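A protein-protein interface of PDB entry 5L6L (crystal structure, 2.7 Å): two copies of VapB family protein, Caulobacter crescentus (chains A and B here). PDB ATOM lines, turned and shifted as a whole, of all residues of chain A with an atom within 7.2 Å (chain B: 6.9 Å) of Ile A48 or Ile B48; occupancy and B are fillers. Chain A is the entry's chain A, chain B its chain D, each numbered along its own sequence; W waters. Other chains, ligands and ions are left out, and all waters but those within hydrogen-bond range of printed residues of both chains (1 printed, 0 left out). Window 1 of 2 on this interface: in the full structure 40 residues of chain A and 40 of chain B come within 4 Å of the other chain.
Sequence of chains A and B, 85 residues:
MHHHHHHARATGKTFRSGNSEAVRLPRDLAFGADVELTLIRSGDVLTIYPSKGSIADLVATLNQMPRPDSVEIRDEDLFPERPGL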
ATOM      1  N   THR A  14     -32.699 -13.431   0.873  1.00  0.00           N
ATOM      2  CA  THR A  14     -31.560 -12.609   1.267  1.00  0.00           C
ATOM      3  C   THR A  14     -31.551 -12.427   2.780  1.00  0.00           C
ATOM      4  O   THR A  14     -32.590 -12.506   3.450  1.00  0.00           O
ATOM      5  CB  THR A  14     -31.580 -11.223   0.594  1.00  0.00           C
ATOM      6  OG1 THR A  14     -32.876 -10.618   0.699  1.00  0.00           O
ATOM      7  CG2 THR A  14     -31.182 -11.304  -0.867  1.00  0.00           C
ATOM      8  N   VAL A  23     -26.260 -14.050   0.465  1.00  0.00           N
ATOM      9  CA  VAL A  23     -27.174 -15.113   0.064  1.00  0.00           C
ATOM     10  C   VAL A  23     -26.533 -16.446   0.406  1.00  0.00           C
ATOM     11  O   VAL A  23     -25.349 -16.655   0.120  1.00  0.00           O
ATOM     12  CB  VAL A  23     -27.498 -15.046  -1.439  1.00  0.00           C
ATOM     13  CG1 VAL A  23     -28.366 -16.204  -1.844  1.00  0.00           C
ATOM     14  CG2 VAL A  23     -28.193 -13.753  -1.740  1.00  0.00           C
ATOM     15  N   ARG A  24     -27.316 -17.346   1.008  1.00  0.00           N
ATOM     16  CA  ARG A  24     -26.836 -18.686   1.344  1.00  0.00           C
ATOM     17  C   ARG A  24     -26.863 -19.607   0.127  1.00  0.00           C
ATOM     18  O   ARG A  24     -27.761 -19.539  -0.720  1.00  0.00           O
ATOM     19  CB  ARG A  24     -27.680 -19.295   2.467  1.00  0.00           C
ATOM     20  CG  ARG A  24     -27.243 -18.912   3.867  1.00  0.00           C
ATOM     21  CD  ARG A  24     -28.186 -19.477   4.922  1.00  0.00           C
ATOM     22  NE  ARG A  24     -29.400 -18.690   4.976  1.00  0.00           N
ATOM     23  CZ  ARG A  24     -29.602 -17.697   5.829  1.00  0.00           C
ATOM     24  NH1 ARG A  24     -28.668 -17.393   6.736  1.00  0.00           N
ATOM     25  NH2 ARG A  24     -30.745 -17.018   5.784  1.00  0.00           N
ATOM     26  N   LEU A  25     -25.863 -20.468   0.043  1.00  0.00           N
ATOM     27  CA  LEU A  25     -25.774 -21.430  -1.039  1.00  0.00           C
ATOM     28  C   LEU A  25     -25.878 -22.822  -0.435  1.00  0.00           C
ATOM     29  O   LEU A  25     -24.980 -23.235   0.318  1.00  0.00           O
ATOM     30  CB  LEU A  25     -24.461 -21.271  -1.805  1.00  0.00           C
ATOM     31  CG  LEU A  25     -24.075 -19.866  -2.289  1.00  0.00           C
ATOM     32  CD1 LEU A  25     -22.734 -19.858  -3.026  1.00  0.00           C
ATOM     33  CD2 LEU A  25     -25.166 -19.276  -3.159  1.00  0.00           C
ATOM     34  N   LEU A  29     -25.434 -26.733  -4.441  1.00  0.00           N
ATOM     35  CA  LEU A  29     -25.212 -25.550  -5.265  1.00  0.00           C
ATOM     36  C   LEU A  29     -23.908 -24.836  -4.949  1.00  0.00           C
ATOM     37  O   LEU A  29     -23.514 -23.942  -5.711  1.00  0.00           O
ATOM     38  CB  LEU A  29     -26.356 -24.537  -5.081  1.00  0.00           C
ATOM     39  CG  LEU A  29     -27.714 -24.806  -5.717  1.00  0.00           C
ATOM     40  CD1 LEU A  29     -28.436 -25.962  -5.055  1.00  0.00           C
ATOM     41  CD2 LEU A  29     -28.531 -23.564  -5.615  1.00  0.00           C
ATOM     42  N   PHE A  31     -20.030 -23.608  -4.220  1.00  0.00           N
ATOM     43  CA  PHE A  31     -18.674 -23.738  -4.718  1.00  0.00           C
ATOM     44  C   PHE A  31     -17.765 -24.010  -3.526  1.00  0.00           C
ATOM     45  O   PHE A  31     -18.198 -24.011  -2.374  1.00  0.00           O
ATOM     46  CB  PHE A  31     -18.238 -22.483  -5.473  1.00  0.00           C
ATOM     47  CG  PHE A  31     -19.143 -22.102  -6.596  1.00  0.00           C
ATOM     48  CD1 PHE A  31     -20.140 -21.168  -6.412  1.00  0.00           C
ATOM     49  CD2 PHE A  31     -18.986 -22.660  -7.846  1.00  0.00           C
ATOM     50  CE1 PHE A  31     -20.981 -20.806  -7.463  1.00  0.00           C
ATOM     51  CE2 PHE A  31     -19.804 -22.291  -8.895  1.00  0.00           C
ATOM     52  CZ  PHE A  31     -20.806 -21.371  -8.707  1.00  0.00           C
ATOM     53  N   LEU A  37     -14.731 -16.371  -7.472  1.00  0.00           N
ATOM     54  CA  LEU A  37     -15.907 -16.323  -8.330  1.00  0.00           C
ATOM     55  C   LEU A  37     -16.087 -14.937  -8.938  1.00  0.00           C
ATOM     56  O   LEU A  37     -15.705 -13.923  -8.342  1.00  0.00           O
ATOM     57  CB  LEU A  37     -17.188 -16.688  -7.562  1.00  0.00           C
ATOM     58  CG  LEU A  37     -17.300 -17.983  -6.755  1.00  0.00           C
ATOM     59  CD1 LEU A  37     -18.501 -17.910  -5.821  1.00  0.00           C
ATOM     60  CD2 LEU A  37     -17.430 -19.188  -7.668  1.00  0.00           C
ATOM     61  N   THR A  38     -16.705 -14.912 -10.120  1.00  0.00           N
ATOM     62  CA  THR A  38     -17.226 -13.688 -10.712  1.00  0.00           C
ATOM     63  C   THR A  38     -18.747 -13.668 -10.584  1.00  0.00           C
ATOM     64  O   THR A  38     -19.414 -14.678 -10.813  1.00  0.00           O
ATOM     65  CB  THR A  38     -16.804 -13.561 -12.179  1.00  0.00           C
ATOM     66  OG1 THR A  38     -15.375 -13.631 -12.262  1.00  0.00           O
ATOM     67  CG2 THR A  38     -17.239 -12.212 -12.750  1.00  0.00           C
ATOM     68  N   LEU A  39     -19.286 -12.515 -10.186  1.00  0.00           N
ATOM     69  CA  LEU A  39     -20.711 -12.320  -9.952  1.00  0.00           C
ATOM     70  C   LEU A  39     -21.196 -11.177 -10.831  1.00  0.00           C
ATOM     71  O   LEU A  39     -20.772 -10.037 -10.649  1.00  0.00           O
ATOM     72  CB  LEU A  39     -20.973 -11.991  -8.482  1.00  0.00           C
ATOM     73  CG  LEU A  39     -20.560 -13.009  -7.425  1.00  0.00           C
ATOM     74  CD1 LEU A  39     -19.110 -12.825  -7.044  1.00  0.00           C
ATOM     75  CD2 LEU A  39     -21.460 -12.898  -6.214  1.00  0.00           C
ATOM     76  N   ILE A  40     -22.082 -11.458 -11.769  1.00  0.00           N
ATOM     77  CA  ILE A  40     -22.547 -10.417 -12.673  1.00  0.00           C
ATOM     78  C   ILE A  40     -24.058 -10.307 -12.567  1.00  0.00           C
ATOM     79  O   ILE A  40     -24.782 -11.293 -12.743  1.00  0.00           O
ATOM     80  CB  ILE A  40     -22.107 -10.661 -14.123  1.00  0.00           C
ATOM     81  CG1 ILE A  40     -20.647 -11.119 -14.170  1.00  0.00           C
ATOM     82  CG2 ILE A  40     -22.241  -9.366 -14.937  1.00  0.00           C
ATOM     83  CD1 ILE A  40     -20.034 -11.031 -15.559  1.00  0.00           C
ATOM     84  N   ASP A  44     -32.320  -7.921 -12.735  1.00  0.00           N
ATOM     85  CA  ASP A  44     -32.261  -8.537 -11.424  1.00  0.00           C
ATOM     86  C   ASP A  44     -31.856 -10.002 -11.503  1.00  0.00           C
ATOM     87  O   ASP A  44     -32.164 -10.774 -10.590  1.00  0.00           O
ATOM     88  CB  ASP A  44     -33.589  -8.362 -10.687  1.00  0.00           C
ATOM     89  CG  ASP A  44     -34.761  -8.964 -11.427  1.00  0.00           C
ATOM     90  OD1 ASP A  44     -34.548  -9.768 -12.363  1.00  0.00           O
ATOM     91  OD2 ASP A  44     -35.904  -8.635 -11.054  1.00  0.00           O
ATOM     92  N   VAL A  45     -31.162 -10.412 -12.575  1.00  0.00           N
ATOM     93  CA  VAL A  45     -30.596 -11.754 -12.646  1.00  0.00           C
ATOM     94  C   VAL A  45     -29.133 -11.699 -12.247  1.00  0.00           C
ATOM     95  O   VAL A  45     -28.357 -10.930 -12.824  1.00  0.00           O
ATOM     96  CB  VAL A  45     -30.751 -12.378 -14.031  1.00  0.00           C
ATOM     97  CG1 VAL A  45     -30.087 -13.738 -14.017  1.00  0.00           C
ATOM     98  CG2 VAL A  45     -32.217 -12.511 -14.379  1.00  0.00           C
ATOM     99  N   LEU A  46     -28.761 -12.515 -11.260  1.00  0.00           N
ATOM    100  CA  LEU A  46     -27.390 -12.636 -10.776  1.00  0.00           C
ATOM    101  C   LEU A  46     -26.775 -13.927 -11.311  1.00  0.00           C
ATOM    102  O   LEU A  46     -27.345 -15.006 -11.140  1.00  0.00           O
ATOM    103  CB  LEU A  46     -27.361 -12.617  -9.235  1.00  0.00           C
ATOM    104  CG  LEU A  46     -25.980 -12.465  -8.576  1.00  0.00           C
ATOM    105  CD1 LEU A  46     -25.268 -11.231  -9.091  1.00  0.00           C
ATOM    106  CD2 LEU A  46     -26.081 -12.391  -7.070  1.00  0.00           C
ATOM    107  N   THR A  47     -25.615 -13.820 -11.953  1.00  0.00           N
ATOM    108  CA  THR A  47     -24.952 -14.960 -12.589  1.00  0.00           C
ATOM    109  C   THR A  47     -23.573 -15.112 -11.982  1.00  0.00           C
ATOM    110  O   THR A  47     -22.735 -14.224 -12.149  1.00  0.00           O
ATOM    111  CB  THR A  47     -24.827 -14.772 -14.101  1.00  0.00           C
ATOM    112  OG1 THR A  47     -26.124 -14.619 -14.690  1.00  0.00           O
ATOM    113  CG2 THR A  47     -24.117 -15.969 -14.743  1.00  0.00           C
ATOM    114  N   ILE A  48     -23.341 -16.234 -11.296  1.00  0.00           N
ATOM    115  CA  ILE A  48     -22.091 -16.526 -10.595  1.00  0.00           C
ATOM    116  C   ILE A  48     -21.401 -17.720 -11.252  1.00  0.00           C
ATOM    117  O   ILE A  48     -22.071 -18.670 -11.685  1.00  0.00           O
ATOM    118  CB  ILE A  48     -22.379 -16.828  -9.118  1.00  0.00           C
ATOM    119  CG1 ILE A  48     -23.271 -15.732  -8.524  1.00  0.00           C
ATOM    120  CG2 ILE A  48     -21.095 -17.006  -8.364  1.00  0.00           C
ATOM    121  CD1 ILE A  48     -23.509 -15.842  -7.031  1.00  0.00           C
ATOM    122  N   TYR A  49     -20.074 -17.682 -11.325  1.00  0.00           N
ATOM    123  CA  TYR A  49     -19.289 -18.789 -11.866  1.00  0.00           C
ATOM    124  C   TYR A  49     -17.820 -18.569 -11.489  1.00  0.00           C
ATOM    125  O   TYR A  49     -17.427 -17.439 -11.173  1.00  0.00           O
ATOM    126  CB  TYR A  49     -19.446 -18.910 -13.398  1.00  0.00           C
ATOM    127  CG  TYR A  49     -19.095 -17.659 -14.158  1.00  0.00           C
ATOM    128  CD1 TYR A  49     -17.766 -17.356 -14.467  1.00  0.00           C
ATOM    129  CD2 TYR A  49     -20.083 -16.773 -14.570  1.00  0.00           C
ATOM    130  CE1 TYR A  49     -17.435 -16.205 -15.165  1.00  0.00           C
ATOM    131  CE2 TYR A  49     -19.753 -15.608 -15.265  1.00  0.00           C
ATOM    132  CZ  TYR A  49     -18.431 -15.338 -15.560  1.00  0.00           C
ATOM    133  OH  TYR A  49     -18.096 -14.194 -16.239  1.00  0.00           O
ATOM    134  N   PRO A  50     -17.003 -19.632 -11.493  1.00  0.00           N
ATOM    135  CA  PRO A  50     -15.594 -19.468 -11.115  1.00  0.00           C
ATOM    136  C   PRO A  50     -14.859 -18.578 -12.104  1.00  0.00           C
ATOM    137  O   PRO A  50     -15.063 -18.672 -13.317  1.00  0.00           O
ATOM    138  CB  PRO A  50     -15.053 -20.904 -11.134  1.00  0.00           C
ATOM    139  CG  PRO A  50     -16.278 -21.771 -10.947  1.00  0.00           C
ATOM    140  CD  PRO A  50     -17.342 -21.051 -11.708  1.00  0.00           C
ATOM    141  N   VAL B  23     -22.360 -16.131  -0.157  1.00  0.00           N
ATOM    142  CA  VAL B  23     -21.722 -15.101  -0.965  1.00  0.00           C
ATOM    143  C   VAL B  23     -22.258 -13.761  -0.498  1.00  0.00           C
ATOM    144  O   VAL B  23     -23.469 -13.609  -0.306  1.00  0.00           O
ATOM    145  CB  VAL B  23     -22.004 -15.302  -2.462  1.00  0.00           C
ATOM    146  CG1 VAL B  23     -21.230 -16.501  -2.981  1.00  0.00           C
ATOM    147  CG2 VAL B  23     -23.490 -15.515  -2.682  1.00  0.00           C
ATOM    148  N   LEU B  25     -23.124  -9.879  -1.220  1.00  0.00           N
ATOM    149  CA  LEU B  25     -23.553  -9.085  -2.359  1.00  0.00           C
ATOM    150  C   LEU B  25     -23.298  -7.618  -2.048  1.00  0.00           C
ATOM    151  O   LEU B  25     -23.944  -7.065  -1.140  1.00  0.00           O
ATOM    152  CB  LEU B  25     -25.031  -9.335  -2.642  1.00  0.00           C
ATOM    153  CG  LEU B  25     -25.467 -10.501  -3.543  1.00  0.00           C
ATOM    154  CD1 LEU B  25     -24.528 -11.709  -3.571  1.00  0.00           C
ATOM    155  CD2 LEU B  25     -26.871 -10.910  -3.145  1.00  0.00           C
ATOM    156  N   PHE B  31     -30.049  -7.801  -4.167  1.00  0.00           N
ATOM    157  CA  PHE B  31     -31.501  -7.737  -4.286  1.00  0.00           C
ATOM    158  C   PHE B  31     -32.005  -6.908  -3.115  1.00  0.00           C
ATOM    159  O   PHE B  31     -31.225  -6.337  -2.352  1.00  0.00           O
ATOM    160  CB  PHE B  31     -32.137  -9.125  -4.293  1.00  0.00           C
ATOM    161  CG  PHE B  31     -31.514 -10.105  -5.261  1.00  0.00           C
ATOM    162  CD1 PHE B  31     -30.442 -10.905  -4.869  1.00  0.00           C
ATOM    163  CD2 PHE B  31     -32.038 -10.278  -6.537  1.00  0.00           C
ATOM    164  CE1 PHE B  31     -29.883 -11.830  -5.736  1.00  0.00           C
ATOM    165  CE2 PHE B  31     -31.475 -11.208  -7.405  1.00  0.00           C
ATOM    166  CZ  PHE B  31     -30.400 -11.988  -6.998  1.00  0.00           C
ATOM    167  N   LEU B  37     -35.748 -15.796  -3.298  1.00  0.00           N
ATOM    168  CA  LEU B  37     -34.867 -16.033  -4.425  1.00  0.00           C
ATOM    169  C   LEU B  37     -35.062 -17.441  -4.951  1.00  0.00           C
ATOM    170  O   LEU B  37     -35.421 -18.361  -4.210  1.00  0.00           O
ATOM    171  CB  LEU B  37     -33.395 -15.835  -4.029  1.00  0.00           C
ATOM    172  CG  LEU B  37     -33.073 -14.457  -3.431  1.00  0.00           C
ATOM    173  CD1 LEU B  37     -31.672 -14.395  -2.839  1.00  0.00           C
ATOM    174  CD2 LEU B  37     -33.265 -13.391  -4.499  1.00  0.00           C
ATOM    175  N   THR B  38     -34.827 -17.589  -6.246  1.00  0.00           N
ATOM    176  CA  THR B  38     -34.679 -18.882  -6.887  1.00  0.00           C
ATOM    177  C   THR B  38     -33.225 -19.005  -7.302  1.00  0.00           C
ATOM    178  O   THR B  38     -32.650 -18.043  -7.835  1.00  0.00           O
ATOM    179  CB  THR B  38     -35.611 -19.004  -8.095  1.00  0.00           C
ATOM    180  OG1 THR B  38     -36.965 -18.991  -7.637  1.00  0.00           O
ATOM    181  CG2 THR B  38     -35.347 -20.304  -8.891  1.00  0.00           C
ATOM    182  N   LEU B  39     -32.628 -20.166  -7.032  1.00  0.00           N
ATOM    183  CA  LEU B  39     -31.233 -20.427  -7.373  1.00  0.00           C
ATOM    184  C   LEU B  39     -31.153 -21.690  -8.214  1.00  0.00           C
ATOM    185  O   LEU B  39     -31.748 -22.713  -7.856  1.00  0.00           O
ATOM    186  CB  LEU B  39     -30.354 -20.603  -6.130  1.00  0.00           C
ATOM    187  CG  LEU B  39     -30.380 -19.620  -4.966  1.00  0.00           C
ATOM    188  CD1 LEU B  39     -31.596 -19.858  -4.092  1.00  0.00           C
ATOM    189  CD2 LEU B  39     -29.121 -19.793  -4.146  1.00  0.00           C
ATOM    190  N   ILE B  40     -30.409 -21.642  -9.312  1.00  0.00           N
ATOM    191  CA  ILE B  40     -30.199 -22.837 -10.119  1.00  0.00           C
ATOM    192  C   ILE B  40     -28.732 -22.918 -10.513  1.00  0.00           C
ATOM    193  O   ILE B  40     -28.115 -21.912 -10.883  1.00  0.00           O
ATOM    194  CB  ILE B  40     -31.122 -22.862 -11.358  1.00  0.00           C
ATOM    195  CG1 ILE B  40     -30.773 -24.037 -12.262  1.00  0.00           C
ATOM    196  CG2 ILE B  40     -31.035 -21.554 -12.134  1.00  0.00           C
ATOM    197  CD1 ILE B  40     -31.688 -24.160 -13.400  1.00  0.00           C
ATOM    198  N   ARG B  41     -28.176 -24.117 -10.425  1.00  0.00           N
ATOM    199  CA  ARG B  41     -26.769 -24.365 -10.682  1.00  0.00           C
ATOM    200  C   ARG B  41     -26.666 -25.443 -11.746  1.00  0.00           C
ATOM    201  O   ARG B  41     -27.171 -26.545 -11.549  1.00  0.00           O
ATOM    202  CB  ARG B  41     -26.072 -24.802  -9.393  1.00  0.00           C
ATOM    203  CG  ARG B  41     -24.682 -25.350  -9.552  1.00  0.00           C
ATOM    204  CD  ARG B  41     -23.724 -24.228  -9.630  1.00  0.00           C
ATOM    205  NE  ARG B  41     -22.393 -24.645 -10.031  1.00  0.00           N
ATOM    206  CZ  ARG B  41     -21.453 -25.043  -9.185  1.00  0.00           C
ATOM    207  NH1 ARG B  41     -20.249 -25.379  -9.641  1.00  0.00           N
ATOM    208  NH2 ARG B  41     -21.718 -25.090  -7.885  1.00  0.00           N
ATOM    209  N   ASP B  44     -20.832 -24.985 -14.394  1.00  0.00           N
ATOM    210  CA  ASP B  44     -20.026 -23.899 -13.849  1.00  0.00           C
ATOM    211  C   ASP B  44     -20.869 -22.780 -13.281  1.00  0.00           C
ATOM    212  O   ASP B  44     -20.350 -21.961 -12.519  1.00  0.00           O
ATOM    213  CB  ASP B  44     -19.126 -23.292 -14.931  1.00  0.00           C
ATOM    214  CG  ASP B  44     -17.978 -24.185 -15.320  1.00  0.00           C
ATOM    215  OD1 ASP B  44     -17.399 -24.823 -14.407  1.00  0.00           O
ATOM    216  OD2 ASP B  44     -17.650 -24.228 -16.534  1.00  0.00           O
ATOM    217  N   VAL B  45     -22.135 -22.691 -13.657  1.00  0.00           N
ATOM    218  CA  VAL B  45     -22.885 -21.449 -13.528  1.00  0.00           C
ATOM    219  C   VAL B  45     -23.913 -21.587 -12.415  1.00  0.00           C
ATOM    220  O   VAL B  45     -24.705 -22.535 -12.416  1.00  0.00           O
ATOM    221  CB  VAL B  45     -23.563 -21.074 -14.862  1.00  0.00           C
ATOM    222  CG1 VAL B  45     -24.306 -19.753 -14.743  1.00  0.00           C
ATOM    223  CG2 VAL B  45     -22.546 -21.008 -15.986  1.00  0.00           C
ATOM    224  N   LEU B  46     -23.922 -20.623 -11.490  1.00  0.00           N
ATOM    225  CA  LEU B  46     -25.024 -20.417 -10.556  1.00  0.00           C
ATOM    226  C   LEU B  46     -25.791 -19.167 -10.961  1.00  0.00           C
ATOM    227  O   LEU B  46     -25.208 -18.083 -11.068  1.00  0.00           O
ATOM    228  CB  LEU B  46     -24.520 -20.265  -9.110  1.00  0.00           C
ATOM    229  CG  LEU B  46     -25.529 -19.971  -7.970  1.00  0.00           C
ATOM    230  CD1 LEU B  46     -26.611 -21.001  -7.876  1.00  0.00           C
ATOM    231  CD2 LEU B  46     -24.835 -19.885  -6.620  1.00  0.00           C
ATOM    232  N   THR B  47     -27.089 -19.314 -11.185  1.00  0.00           N
ATOM    233  CA  THR B  47     -27.967 -18.186 -11.458  1.00  0.00           C
ATOM    234  C   THR B  47     -28.943 -17.992 -10.303  1.00  0.00           C
ATOM    235  O   THR B  47     -29.548 -18.962  -9.823  1.00  0.00           O
ATOM    236  CB  THR B  47     -28.731 -18.398 -12.761  1.00  0.00           C
ATOM    237  OG1 THR B  47     -27.816 -18.319 -13.853  1.00  0.00           O
ATOM    238  CG2 THR B  47     -29.817 -17.351 -12.931  1.00  0.00           C
ATOM    239  N   ILE B  48     -29.079 -16.742  -9.858  1.00  0.00           N
ATOM    240  CA  ILE B  48     -29.935 -16.363  -8.737  1.00  0.00           C
ATOM    241  C   ILE B  48     -30.833 -15.215  -9.180  1.00  0.00           C
ATOM    242  O   ILE B  48     -30.348 -14.199  -9.693  1.00  0.00           O
ATOM    243  CB  ILE B  48     -29.115 -15.939  -7.508  1.00  0.00           C
ATOM    244  CG1 ILE B  48     -28.099 -17.008  -7.128  1.00  0.00           C
ATOM    245  CG2 ILE B  48     -30.026 -15.662  -6.337  1.00  0.00           C
ATOM    246  CD1 ILE B  48     -27.177 -16.587  -6.013  1.00  0.00           C
ATOM    247  N   TYR B  49     -32.132 -15.353  -8.963  1.00  0.00           N
ATOM    248  CA  TYR B  49     -33.034 -14.302  -9.398  1.00  0.00           C
ATOM    249  C   TYR B  49     -34.286 -14.356  -8.546  1.00  0.00           C
ATOM    250  O   TYR B  49     -34.622 -15.414  -7.993  1.00  0.00           O
ATOM    251  CB  TYR B  49     -33.377 -14.450 -10.887  1.00  0.00           C
ATOM    252  CG  TYR B  49     -34.090 -15.740 -11.189  1.00  0.00           C
ATOM    253  CD1 TYR B  49     -33.389 -16.860 -11.644  1.00  0.00           C
ATOM    254  CD2 TYR B  49     -35.465 -15.848 -11.014  1.00  0.00           C
ATOM    255  CE1 TYR B  49     -34.041 -18.051 -11.905  1.00  0.00           C
ATOM    256  CE2 TYR B  49     -36.126 -17.040 -11.265  1.00  0.00           C
ATOM    257  CZ  TYR B  49     -35.414 -18.131 -11.710  1.00  0.00           C
ATOM    258  OH  TYR B  49     -36.086 -19.297 -11.973  1.00  0.00           O
ATOM    259  N   PRO B  50     -35.004 -13.247  -8.413  1.00  0.00           N
ATOM    260  CA  PRO B  50     -36.219 -13.245  -7.583  1.00  0.00           C
ATOM    261  C   PRO B  50     -37.259 -14.241  -8.084  1.00  0.00           C
ATOM    262  O   PRO B  50     -37.476 -14.391  -9.289  1.00  0.00           O
ATOM    263  CB  PRO B  50     -36.734 -11.806  -7.702  1.00  0.00           C
ATOM    264  CG  PRO B  50     -35.541 -11.003  -8.231  1.00  0.00           C
ATOM    265  CD  PRO B  50     -34.721 -11.934  -9.021  1.00  0.00           C
HETATM  266  O   HOH W   1     -27.437 -16.636 -15.587  1.00  0.00           O
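The backbone NH (N) of Val A23 is in hydrogen-bond range of the backbone carbonyl oxygen (O) of Val B23.
O of Leu A29 is in hydrogen-bond range of NH2 of Arg B41 (3.0 Å).
The backbone NH of Ile B48 sits at hydrogen-bond distance from the backbone carbonyl oxygen of Leu A46 (2.8 Å).
The backbone NH (N) of Ile A48 lies within hydrogen-bond range of the backbone carbonyl oxygen (O) of Leu B46 (2.6 Å).
O of Tyr A49 is in hydrogen-bond range of N of Thr A38.
O of Ile A40 is in hydrogen-bond range of N of Thr A47, at 2.8 Å.
N of Thr B38 is in hydrogen-bond range of O of Tyr B49, at 2.8 Å.
N of Thr B47 lies within hydrogen-bond range of O of Ile B40 (2.8 Å).
Among the printed residues, pairs that only touch across the chains: Phe A31 with Arg B41, Asp A44 with Pro B50, Pro A50 with Asp B44, Leu A46 with Thr B47, Asp A44 with Phe B31, Tyr A49 with Asp B44, Ile A48 with Val B45, Val A23 with Leu B25, Thr A47 with Leu B46, Leu A29 with Leu B39, Leu A25 with Leu B46, Leu A25 with Val B23, Phe A31 with Asp B44, Arg A24 with Leu B39, Thr A14 with Leu B37, Val A23 with Leu B37, Leu A46 with Leu B46, Val A45 with Ile B48, Val A45 with Thr B47, Thr A47 with Val B45, Ile A48 with Asp B44, Asp A44 with Tyr B49, Leu A46 with Phe B31, Ile A48 with Ile B48, Leu A46 with Leu B25, Phe A31 with Leu B46, Leu A29 with Leu B46 and Asp A44 with Ile B48.
Of the printed residues of chain B, Thr A47 touches Val B45 and Leu B46.
Ile A48 touches just these residues of chain B: Asp B44, Val B45, Leu B46 and Ile B48.
Of the printed residues of chain A, Phe B31 touches Asp A44 (3.3 Å) and Leu A46 (3.8 Å).
Of the printed residues of chain A, Thr B47 touches Val A45 and Leu A46.
Ile B48 touches just these residues of chain A: Asp A44 (3.98 Å), Val A45 (3.8 Å), Leu A46 (2.8 Å) and Ile A48 (3.9 Å).
The nearest residue of chain B that does not touch Ile A48 is Val B23 (4.4 Å).
Printed residues of chain A that touch a printed residue of chain B: Thr A14, Val A23, Arg A24, Leu A25, Leu A29, Phe A31, Asp A44, Val A45, Leu A46, Thr A47, Ile A48, Tyr A49 and Pro A50.
Hydrophobic or aromatic side chains of chain A within 4 Å of the printed part of chain B: Val A23, Leu A25, Leu A29, Phe A31, Val A45, Leu A46, Ile A48, Tyr A49 and Pro A50.
Hydrophobic or aromatic side chains of chain B within 4 Å of the printed part of chain A: Val B23, Leu B25, Phe B31, Leu B37, Leu B39, Val B45, Leu B46, Ile B48, Tyr B49 and Pro B50.
Among the printed residues, 32 pairs touch across the chains.
Among the printed residues, no Asp or Glu carboxylate lies within 4 Å of a Lys or Arg side-chain nitrogen of the other chain.
Val A23 touches Leu B25, and with the chains exchanged Leu A25 touches Val B23.
Asp A44 touches Pro B50, and with the chains exchanged Pro A50 touches Asp B44.
Val A45 touches Ile B48, and with the chains exchanged Ile A48 touches Val B45.
Leu A46 touches its own counterpart, Leu B46.
Positions printed for both chains: 23, 25, 31, 37, 38, 39, 40, 44, 45, 46, 47, 48, 49 and 50.
Of the 32 pairs that touch across the chains among the printed residues, 25 have their exchanged pair printed and touching as well.
Water W1 bridges OG1 of Thr B47 (2.4 Å) and OG1 of Thr A47 (2.6 Å).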
